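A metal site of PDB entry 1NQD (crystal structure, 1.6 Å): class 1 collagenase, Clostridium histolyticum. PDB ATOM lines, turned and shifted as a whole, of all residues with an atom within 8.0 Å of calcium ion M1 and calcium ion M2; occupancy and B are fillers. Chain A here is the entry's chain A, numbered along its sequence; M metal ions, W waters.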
ATOM      1  N   GLU A  13       2.263  12.951  -4.042  1.00  0.00           N
ATOM      2  CA  GLU A  13       1.782  13.469  -5.331  1.00  0.00           C
ATOM      3  C   GLU A  13       1.661  14.972  -5.284  1.00  0.00           C
ATOM      4  O   GLU A  13       1.679  15.564  -4.198  1.00  0.00           O
ATOM      5  CB  GLU A  13       0.426  12.809  -5.666  1.00  0.00           C
ATOM      6  CG  GLU A  13      -0.643  13.208  -4.663  1.00  0.00           C
ATOM      7  CD  GLU A  13      -2.043  12.789  -5.118  1.00  0.00           C
ATOM      8  OE1 GLU A  13      -2.438  13.173  -6.237  1.00  0.00           O
ATOM      9  OE2 GLU A  13      -2.840  12.453  -4.207  1.00  0.00           O
ATOM     10  N   LYS A  14       1.524  15.656  -6.421  1.00  0.00           N
ATOM     11  CA  LYS A  14       1.286  17.104  -6.417  1.00  0.00           C
ATOM     12  C   LYS A  14       0.069  17.437  -7.271  1.00  0.00           C
ATOM     13  O   LYS A  14       0.079  17.407  -8.497  1.00  0.00           O
ATOM     14  CB  LYS A  14       2.528  17.868  -6.871  1.00  0.00           C
ATOM     15  CG  LYS A  14       3.826  17.483  -6.178  1.00  0.00           C
ATOM     16  CD  LYS A  14       4.011  18.146  -4.823  1.00  0.00           C
ATOM     17  CE  LYS A  14       3.908  17.133  -3.686  1.00  0.00           C
ATOM     18  NZ  LYS A  14       4.707  17.565  -2.497  1.00  0.00           N
ATOM     19  N   GLU A  15      -1.072  17.738  -6.620  1.00  0.00           N
ATOM     20  CA  GLU A  15      -2.224  18.150  -7.401  1.00  0.00           C
ATOM     21  C   GLU A  15      -2.028  19.587  -7.934  1.00  0.00           C
ATOM     22  O   GLU A  15      -1.269  20.302  -7.266  1.00  0.00           O
ATOM     23  CB  GLU A  15      -3.518  18.137  -6.570  1.00  0.00           C
ATOM     24  CG  GLU A  15      -3.922  16.751  -6.073  1.00  0.00           C
ATOM     25  CD  GLU A  15      -4.629  15.922  -7.126  1.00  0.00           C
ATOM     26  OE1 GLU A  15      -4.921  16.409  -8.232  1.00  0.00           O
ATOM     27  OE2 GLU A  15      -4.861  14.720  -6.839  1.00  0.00           O
ATOM     28  N   ASN A  16      -2.675  19.955  -9.017  1.00  0.00           N
ATOM     29  CA  ASN A  16      -3.568  19.164  -9.824  1.00  0.00           C
ATOM     30  C   ASN A  16      -2.784  18.269 -10.787  1.00  0.00           C
ATOM     31  O   ASN A  16      -1.901  18.766 -11.496  1.00  0.00           O
ATOM     32  CB  ASN A  16      -4.521  20.040 -10.655  1.00  0.00           C
ATOM     33  CG  ASN A  16      -5.536  19.215 -11.408  1.00  0.00           C
ATOM     34  OD1 ASN A  16      -5.253  18.559 -12.417  1.00  0.00           O
ATOM     35  ND2 ASN A  16      -6.776  19.229 -10.914  1.00  0.00           N
ATOM     36  N   ASN A  17      -3.099  16.985 -10.777  1.00  0.00           N
ATOM     37  CA  ASN A  17      -2.412  16.095 -11.722  1.00  0.00           C
ATOM     38  C   ASN A  17      -3.429  15.300 -12.510  1.00  0.00           C
ATOM     39  O   ASN A  17      -3.266  14.114 -12.791  1.00  0.00           O
ATOM     40  CB  ASN A  17      -1.473  15.166 -10.942  1.00  0.00           C
ATOM     41  CG  ASN A  17      -2.184  14.454  -9.799  1.00  0.00           C
ATOM     42  OD1 ASN A  17      -3.417  14.381  -9.773  1.00  0.00           O
ATOM     43  ND2 ASN A  17      -1.387  13.903  -8.877  1.00  0.00           N
ATOM     44  N   ASP A  18      -4.550  15.942 -12.906  1.00  0.00           N
ATOM     45  CA  ASP A  18      -5.575  15.081 -13.482  1.00  0.00           C
ATOM     46  C   ASP A  18      -5.384  14.810 -14.967  1.00  0.00           C
ATOM     47  O   ASP A  18      -6.200  14.090 -15.559  1.00  0.00           O
ATOM     48  CB  ASP A  18      -6.960  15.692 -13.179  1.00  0.00           C
ATOM     49  CG  ASP A  18      -7.161  15.946 -11.697  1.00  0.00           C
ATOM     50  OD1 ASP A  18      -8.017  16.767 -11.287  1.00  0.00           O
ATOM     51  OD2 ASP A  18      -6.467  15.318 -10.866  1.00  0.00           O
ATOM     52  N   SER A  19      -4.334  15.319 -15.614  1.00  0.00           N
ATOM     53  CA  SER A  19      -4.124  15.014 -17.026  1.00  0.00           C
ATOM     54  C   SER A  19      -2.621  14.920 -17.290  1.00  0.00           C
ATOM     55  O   SER A  19      -1.828  15.308 -16.438  1.00  0.00           O
ATOM     56  CB  SER A  19      -4.788  16.055 -17.936  1.00  0.00           C
ATOM     57  OG  SER A  19      -4.296  17.327 -17.572  1.00  0.00           O
ATOM     58  N   LYS A  22      -0.108  17.580 -16.714  1.00  0.00           N
ATOM     59  CA  LYS A  22       0.099  17.946 -15.321  1.00  0.00           C
ATOM     60  C   LYS A  22       0.584  16.788 -14.432  1.00  0.00           C
ATOM     61  O   LYS A  22       0.501  16.813 -13.212  1.00  0.00           O
ATOM     62  CB  LYS A  22      -1.197  18.519 -14.736  1.00  0.00           C
ATOM     63  CG  LYS A  22      -1.587  19.837 -15.382  1.00  0.00           C
ATOM     64  CD  LYS A  22      -3.054  20.153 -15.115  1.00  0.00           C
ATOM     65  CE  LYS A  22      -3.650  21.037 -16.207  1.00  0.00           C
ATOM     66  NZ  LYS A  22      -3.328  22.475 -15.990  1.00  0.00           N
ATOM     67  N   THR A  24       2.498  14.177 -12.151  1.00  0.00           N
ATOM     68  CA  THR A  24       3.498  14.254 -11.093  1.00  0.00           C
ATOM     69  C   THR A  24       4.702  13.409 -11.473  1.00  0.00           C
ATOM     70  O   THR A  24       4.456  12.252 -11.820  1.00  0.00           O
ATOM     71  CB  THR A  24       2.929  13.689  -9.786  1.00  0.00           C
ATOM     72  OG1 THR A  24       1.899  14.575  -9.329  1.00  0.00           O
ATOM     73  CG2 THR A  24       3.958  13.600  -8.662  1.00  0.00           C
ATOM     74  N   GLN A  34       3.146   8.706  -2.601  1.00  0.00           N
ATOM     75  CA  GLN A  34       1.929   8.632  -1.798  1.00  0.00           C
ATOM     76  C   GLN A  34       0.819   9.471  -2.442  1.00  0.00           C
ATOM     77  O   GLN A  34       1.020  10.629  -2.777  1.00  0.00           O
ATOM     78  CB  GLN A  34       2.142   9.128  -0.368  1.00  0.00           C
ATOM     79  CG  GLN A  34       3.035   8.205   0.458  1.00  0.00           C
ATOM     80  CD  GLN A  34       2.980   8.517   1.941  1.00  0.00           C
ATOM     81  OE1 GLN A  34       3.598   7.821   2.743  1.00  0.00           O
ATOM     82  NE2 GLN A  34       2.245   9.570   2.288  1.00  0.00           N
ATOM     83  N   GLY A  35      -0.362   8.851  -2.566  1.00  0.00           N
ATOM     84  CA  GLY A  35      -1.436   9.675  -3.102  1.00  0.00           C
ATOM     85  C   GLY A  35      -2.795   9.280  -2.531  1.00  0.00           C
ATOM     86  O   GLY A  35      -2.940   8.369  -1.727  1.00  0.00           O
ATOM     87  N   SER A  36      -3.796  10.036  -2.974  1.00  0.00           N
ATOM     88  CA  SER A  36      -5.153   9.752  -2.522  1.00  0.00           C
ATOM     89  C   SER A  36      -6.118  10.141  -3.650  1.00  0.00           C
ATOM     90  O   SER A  36      -5.812  11.008  -4.453  1.00  0.00           O
ATOM     91  CB  SER A  36      -5.488  10.418  -1.200  1.00  0.00           C
ATOM     92  OG  SER A  36      -5.610  11.820  -1.368  1.00  0.00           O
ATOM     93  N   LEU A  37      -7.258   9.488  -3.640  1.00  0.00           N
ATOM     94  CA  LEU A  37      -8.349   9.764  -4.577  1.00  0.00           C
ATOM     95  C   LEU A  37      -9.636   9.851  -3.746  1.00  0.00           C
ATOM     96  O   LEU A  37     -10.425   8.916  -3.761  1.00  0.00           O
ATOM     97  CB  LEU A  37      -8.450   8.739  -5.697  1.00  0.00           C
ATOM     98  CG  LEU A  37      -7.205   8.594  -6.598  1.00  0.00           C
ATOM     99  CD1 LEU A  37      -7.138   7.200  -7.182  1.00  0.00           C
ATOM    100  CD2 LEU A  37      -7.253   9.641  -7.717  1.00  0.00           C
ATOM    101  N   LEU A  38      -9.802  10.987  -3.085  1.00  0.00           N
ATOM    102  CA  LEU A  38     -10.933  11.268  -2.205  1.00  0.00           C
ATOM    103  C   LEU A  38     -12.002  12.043  -2.946  1.00  0.00           C
ATOM    104  O   LEU A  38     -11.698  12.990  -3.671  1.00  0.00           O
ATOM    105  CB  LEU A  38     -10.474  12.068  -0.985  1.00  0.00           C
ATOM    106  CG  LEU A  38      -9.319  11.401  -0.207  1.00  0.00           C
ATOM    107  CD1 LEU A  38      -8.889  12.296   0.953  1.00  0.00           C
ATOM    108  CD2 LEU A  38      -9.739  10.019   0.252  1.00  0.00           C
ATOM    109  N   ASP A  40     -14.238  13.800  -5.546  1.00  0.00           N
ATOM    110  CA  ASP A  40     -14.228  13.935  -6.994  1.00  0.00           C
ATOM    111  C   ASP A  40     -12.814  13.976  -7.562  1.00  0.00           C
ATOM    112  O   ASP A  40     -12.692  14.214  -8.760  1.00  0.00           O
ATOM    113  CB  ASP A  40     -15.025  15.165  -7.424  1.00  0.00           C
ATOM    114  CG  ASP A  40     -14.490  16.494  -6.990  1.00  0.00           C
ATOM    115  OD1 ASP A  40     -13.288  16.633  -6.692  1.00  0.00           O
ATOM    116  OD2 ASP A  40     -15.299  17.463  -6.931  1.00  0.00           O
ATOM    117  N   ASP A  41     -11.820  13.699  -6.720  1.00  0.00           N
ATOM    118  CA  ASP A  41     -10.462  13.490  -7.193  1.00  0.00           C
ATOM    119  C   ASP A  41     -10.358  12.006  -7.574  1.00  0.00           C
ATOM    120  O   ASP A  41     -10.127  11.174  -6.690  1.00  0.00           O
ATOM    121  CB  ASP A  41      -9.404  13.863  -6.169  1.00  0.00           C
ATOM    122  CG  ASP A  41      -7.981  13.660  -6.686  1.00  0.00           C
ATOM    123  OD1 ASP A  41      -7.763  13.871  -7.898  1.00  0.00           O
ATOM    124  OD2 ASP A  41      -7.081  13.274  -5.912  1.00  0.00           O
ATOM    125  N   SER A  42     -10.569  11.703  -8.851  1.00  0.00           N
ATOM    126  CA  SER A  42     -10.671  10.336  -9.315  1.00  0.00           C
ATOM    127  C   SER A  42      -9.504   9.935 -10.223  1.00  0.00           C
ATOM    128  O   SER A  42      -9.489   8.770 -10.622  1.00  0.00           O
ATOM    129  CB  SER A  42     -11.955  10.084 -10.112  1.00  0.00           C
ATOM    130  OG  SER A  42     -12.066  10.924 -11.239  1.00  0.00           O
ATOM    131  N   ARG A  43      -8.636  10.891 -10.517  1.00  0.00           N
ATOM    132  CA  ARG A  43      -7.518  10.606 -11.398  1.00  0.00           C
ATOM    133  C   ARG A  43      -6.258  11.294 -10.917  1.00  0.00           C
ATOM    134  O   ARG A  43      -6.274  12.485 -10.594  1.00  0.00           O
ATOM    135  CB  ARG A  43      -7.797  11.085 -12.844  1.00  0.00           C
ATOM    136  CG  ARG A  43      -9.158  10.633 -13.370  1.00  0.00           C
ATOM    137  CD  ARG A  43      -9.593  11.392 -14.593  1.00  0.00           C
ATOM    138  NE  ARG A  43      -8.607  11.611 -15.634  1.00  0.00           N
ATOM    139  CZ  ARG A  43      -8.469  10.940 -16.769  1.00  0.00           C
ATOM    140  NH1 ARG A  43      -9.241   9.912 -17.112  1.00  0.00           N
ATOM    141  NH2 ARG A  43      -7.499  11.318 -17.602  1.00  0.00           N
ATOM    142  N   ASP A  44      -5.161  10.523 -10.904  1.00  0.00           N
ATOM    143  CA  ASP A  44      -3.855  11.078 -10.537  1.00  0.00           C
ATOM    144  C   ASP A  44      -2.829  10.626 -11.568  1.00  0.00           C
ATOM    145  O   ASP A  44      -2.545   9.412 -11.670  1.00  0.00           O
ATOM    146  CB  ASP A  44      -3.430  10.577  -9.167  1.00  0.00           C
ATOM    147  CG  ASP A  44      -4.200  11.115  -7.983  1.00  0.00           C
ATOM    148  OD1 ASP A  44      -4.865  12.164  -8.113  1.00  0.00           O
ATOM    149  OD2 ASP A  44      -3.953  10.608  -6.878  1.00  0.00           O
ATOM    150  N   TYR A  45      -2.292  11.538 -12.359  1.00  0.00           N
ATOM    151  CA  TYR A  45      -1.319  11.185 -13.397  1.00  0.00           C
ATOM    152  C   TYR A  45       0.103  11.317 -12.881  1.00  0.00           C
ATOM    153  O   TYR A  45       0.474  12.265 -12.187  1.00  0.00           O
ATOM    154  CB  TYR A  45      -1.442  12.064 -14.638  1.00  0.00           C
ATOM    155  CG  TYR A  45      -1.923  11.361 -15.877  1.00  0.00           C
ATOM    156  CD1 TYR A  45      -3.123  11.690 -16.497  1.00  0.00           C
ATOM    157  CD2 TYR A  45      -1.160  10.352 -16.442  1.00  0.00           C
ATOM    158  CE1 TYR A  45      -3.541  11.027 -17.629  1.00  0.00           C
ATOM    159  CE2 TYR A  45      -1.563   9.690 -17.565  1.00  0.00           C
ATOM    160  CZ  TYR A  45      -2.757  10.024 -18.164  1.00  0.00           C
ATOM    161  OH  TYR A  45      -3.121   9.331 -19.297  1.00  0.00           O
ATOM    162  N   TYR A  46       0.889  10.312 -13.273  1.00  0.00           N
ATOM    163  CA  TYR A  46       2.315  10.320 -12.999  1.00  0.00           C
ATOM    164  C   TYR A  46       3.087  10.090 -14.303  1.00  0.00           C
ATOM    165  O   TYR A  46       2.559   9.599 -15.279  1.00  0.00           O
ATOM    166  CB  TYR A  46       2.691   9.207 -12.020  1.00  0.00           C
ATOM    167  CG  TYR A  46       2.061   9.313 -10.650  1.00  0.00           C
ATOM    168  CD1 TYR A  46       0.762   8.828 -10.430  1.00  0.00           C
ATOM    169  CD2 TYR A  46       2.762   9.893  -9.607  1.00  0.00           C
ATOM    170  CE1 TYR A  46       0.270   8.965  -9.146  1.00  0.00           C
ATOM    171  CE2 TYR A  46       2.262  10.032  -8.312  1.00  0.00           C
ATOM    172  CZ  TYR A  46       0.969   9.549  -8.122  1.00  0.00           C
ATOM    173  OH  TYR A  46       0.428   9.649  -6.873  1.00  0.00           O
ATOM    174  N   LEU A 106      -1.535   6.590 -15.380  1.00  0.00           N
ATOM    175  CA  LEU A 106      -2.780   7.137 -14.876  1.00  0.00           C
ATOM    176  C   LEU A 106      -3.280   6.241 -13.746  1.00  0.00           C
ATOM    177  O   LEU A 106      -3.629   5.087 -14.044  1.00  0.00           O
ATOM    178  CB  LEU A 106      -3.763   7.196 -16.040  1.00  0.00           C
ATOM    179  CG  LEU A 106      -5.200   7.590 -15.646  1.00  0.00           C
ATOM    180  CD1 LEU A 106      -5.140   8.912 -14.912  1.00  0.00           C
ATOM    181  CD2 LEU A 106      -6.096   7.624 -16.883  1.00  0.00           C
ATOM    182  N   VAL A 107      -3.299   6.764 -12.539  1.00  0.00           N
ATOM    183  CA  VAL A 107      -3.931   6.059 -11.420  1.00  0.00           C
ATOM    184  C   VAL A 107      -5.357   6.602 -11.333  1.00  0.00           C
ATOM    185  O   VAL A 107      -5.538   7.816 -11.291  1.00  0.00           O
ATOM    186  CB  VAL A 107      -3.207   6.280 -10.106  1.00  0.00           C
ATOM    187  CG1 VAL A 107      -3.895   5.640  -8.919  1.00  0.00           C
ATOM    188  CG2 VAL A 107      -1.780   5.732 -10.174  1.00  0.00           C
ATOM    189  N   GLY A 114     -10.206   6.680  -1.501  1.00  0.00           N
ATOM    190  CA  GLY A 114      -9.203   6.132  -0.584  1.00  0.00           C
ATOM    191  C   GLY A 114      -7.780   6.593  -0.931  1.00  0.00           C
ATOM    192  O   GLY A 114      -7.589   7.471  -1.765  1.00  0.00           O
ATOM    193  N   TYR A 116      -3.456   5.434  -1.537  1.00  0.00           N
ATOM    194  CA  TYR A 116      -2.616   4.416  -2.161  1.00  0.00           C
ATOM    195  C   TYR A 116      -1.160   4.853  -2.137  1.00  0.00           C
ATOM    196  O   TYR A 116      -0.883   6.023  -1.901  1.00  0.00           O
ATOM    197  CB  TYR A 116      -3.029   4.140  -3.623  1.00  0.00           C
ATOM    198  CG  TYR A 116      -2.860   5.410  -4.444  1.00  0.00           C
ATOM    199  CD1 TYR A 116      -1.673   5.610  -5.146  1.00  0.00           C
ATOM    200  CD2 TYR A 116      -3.833   6.402  -4.533  1.00  0.00           C
ATOM    201  CE1 TYR A 116      -1.469   6.745  -5.896  1.00  0.00           C
ATOM    202  CE2 TYR A 116      -3.625   7.547  -5.291  1.00  0.00           C
ATOM    203  CZ  TYR A 116      -2.442   7.713  -5.979  1.00  0.00           C
ATOM    204  OH  TYR A 116      -2.203   8.852  -6.732  1.00  0.00           O
HETATM  205 CA    CA M   1      -4.811  12.782  -5.723  1.00  0.00          CA
HETATM  206 CA    CA M   2      -5.654  14.108  -9.101  1.00  0.00          CA
HETATM  207  O   HOH W   1      -5.051  14.431  -3.884  1.00  0.00           O
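Calcium ion M2 is bound by OD2 of Asp 18 (2.3 Å), O of Arg 43 (2.3 Å), OD1 of Asp 44 (2.3 Å), OD1 of Asn 17 (2.4 Å), OD1 of Asp 41 (2.4 Å), OE2 of Glu 15 (2.5 Å) and OE1 of Glu 15 (2.6 Å). Calcium ion M2 has seven donor atoms within binding distance.
The backbone NH of Asp 18 lies within hydrogen-bond range of the side-chain amide oxygen of Asn 16 (2.8 Å). OD2 of Asp 44 sits close to OH of Tyr 116, 2.5 Å away. The backbone NH of Asp 44 is in hydrogen-bond range of the backbone carbonyl oxygen of Val 107, at 2.8 Å. ND2 of Asn 17 sits close to OE1 of Glu 13, at 2.9 Å. O of Asn 17 is in hydrogen-bond range of N of Tyr 45 (2.8 Å). The side-chain amide nitrogen (ND2) of Asn 17 lies within hydrogen-bond range of the side-chain hydroxyl (OG1) of Thr 24, at 3.4 Å. The backbone NH of Glu 13 sits at hydrogen-bond distance from the backbone carbonyl oxygen of Gln 34 (2.9 Å).
Calcium ion M1 is bound by OE2 of Glu 15, OD2 of Asp 41, O of Ser 36, OE1 of Glu 13, OD1 of Asp 44, water W1, OE2 of Glu 13 and OD2 of Asp 44. Calcium ion M1 has eight donor atoms within binding distance.
Of the 25 residues printed, 5 come within 4 Å of calcium ion M1. The nearest printed residue that does not touch calcium ion M1 is Leu 37 (4.5 Å).
The nearest printed residue that does not touch calcium ion M2 is Glu 13 (4.4 Å).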
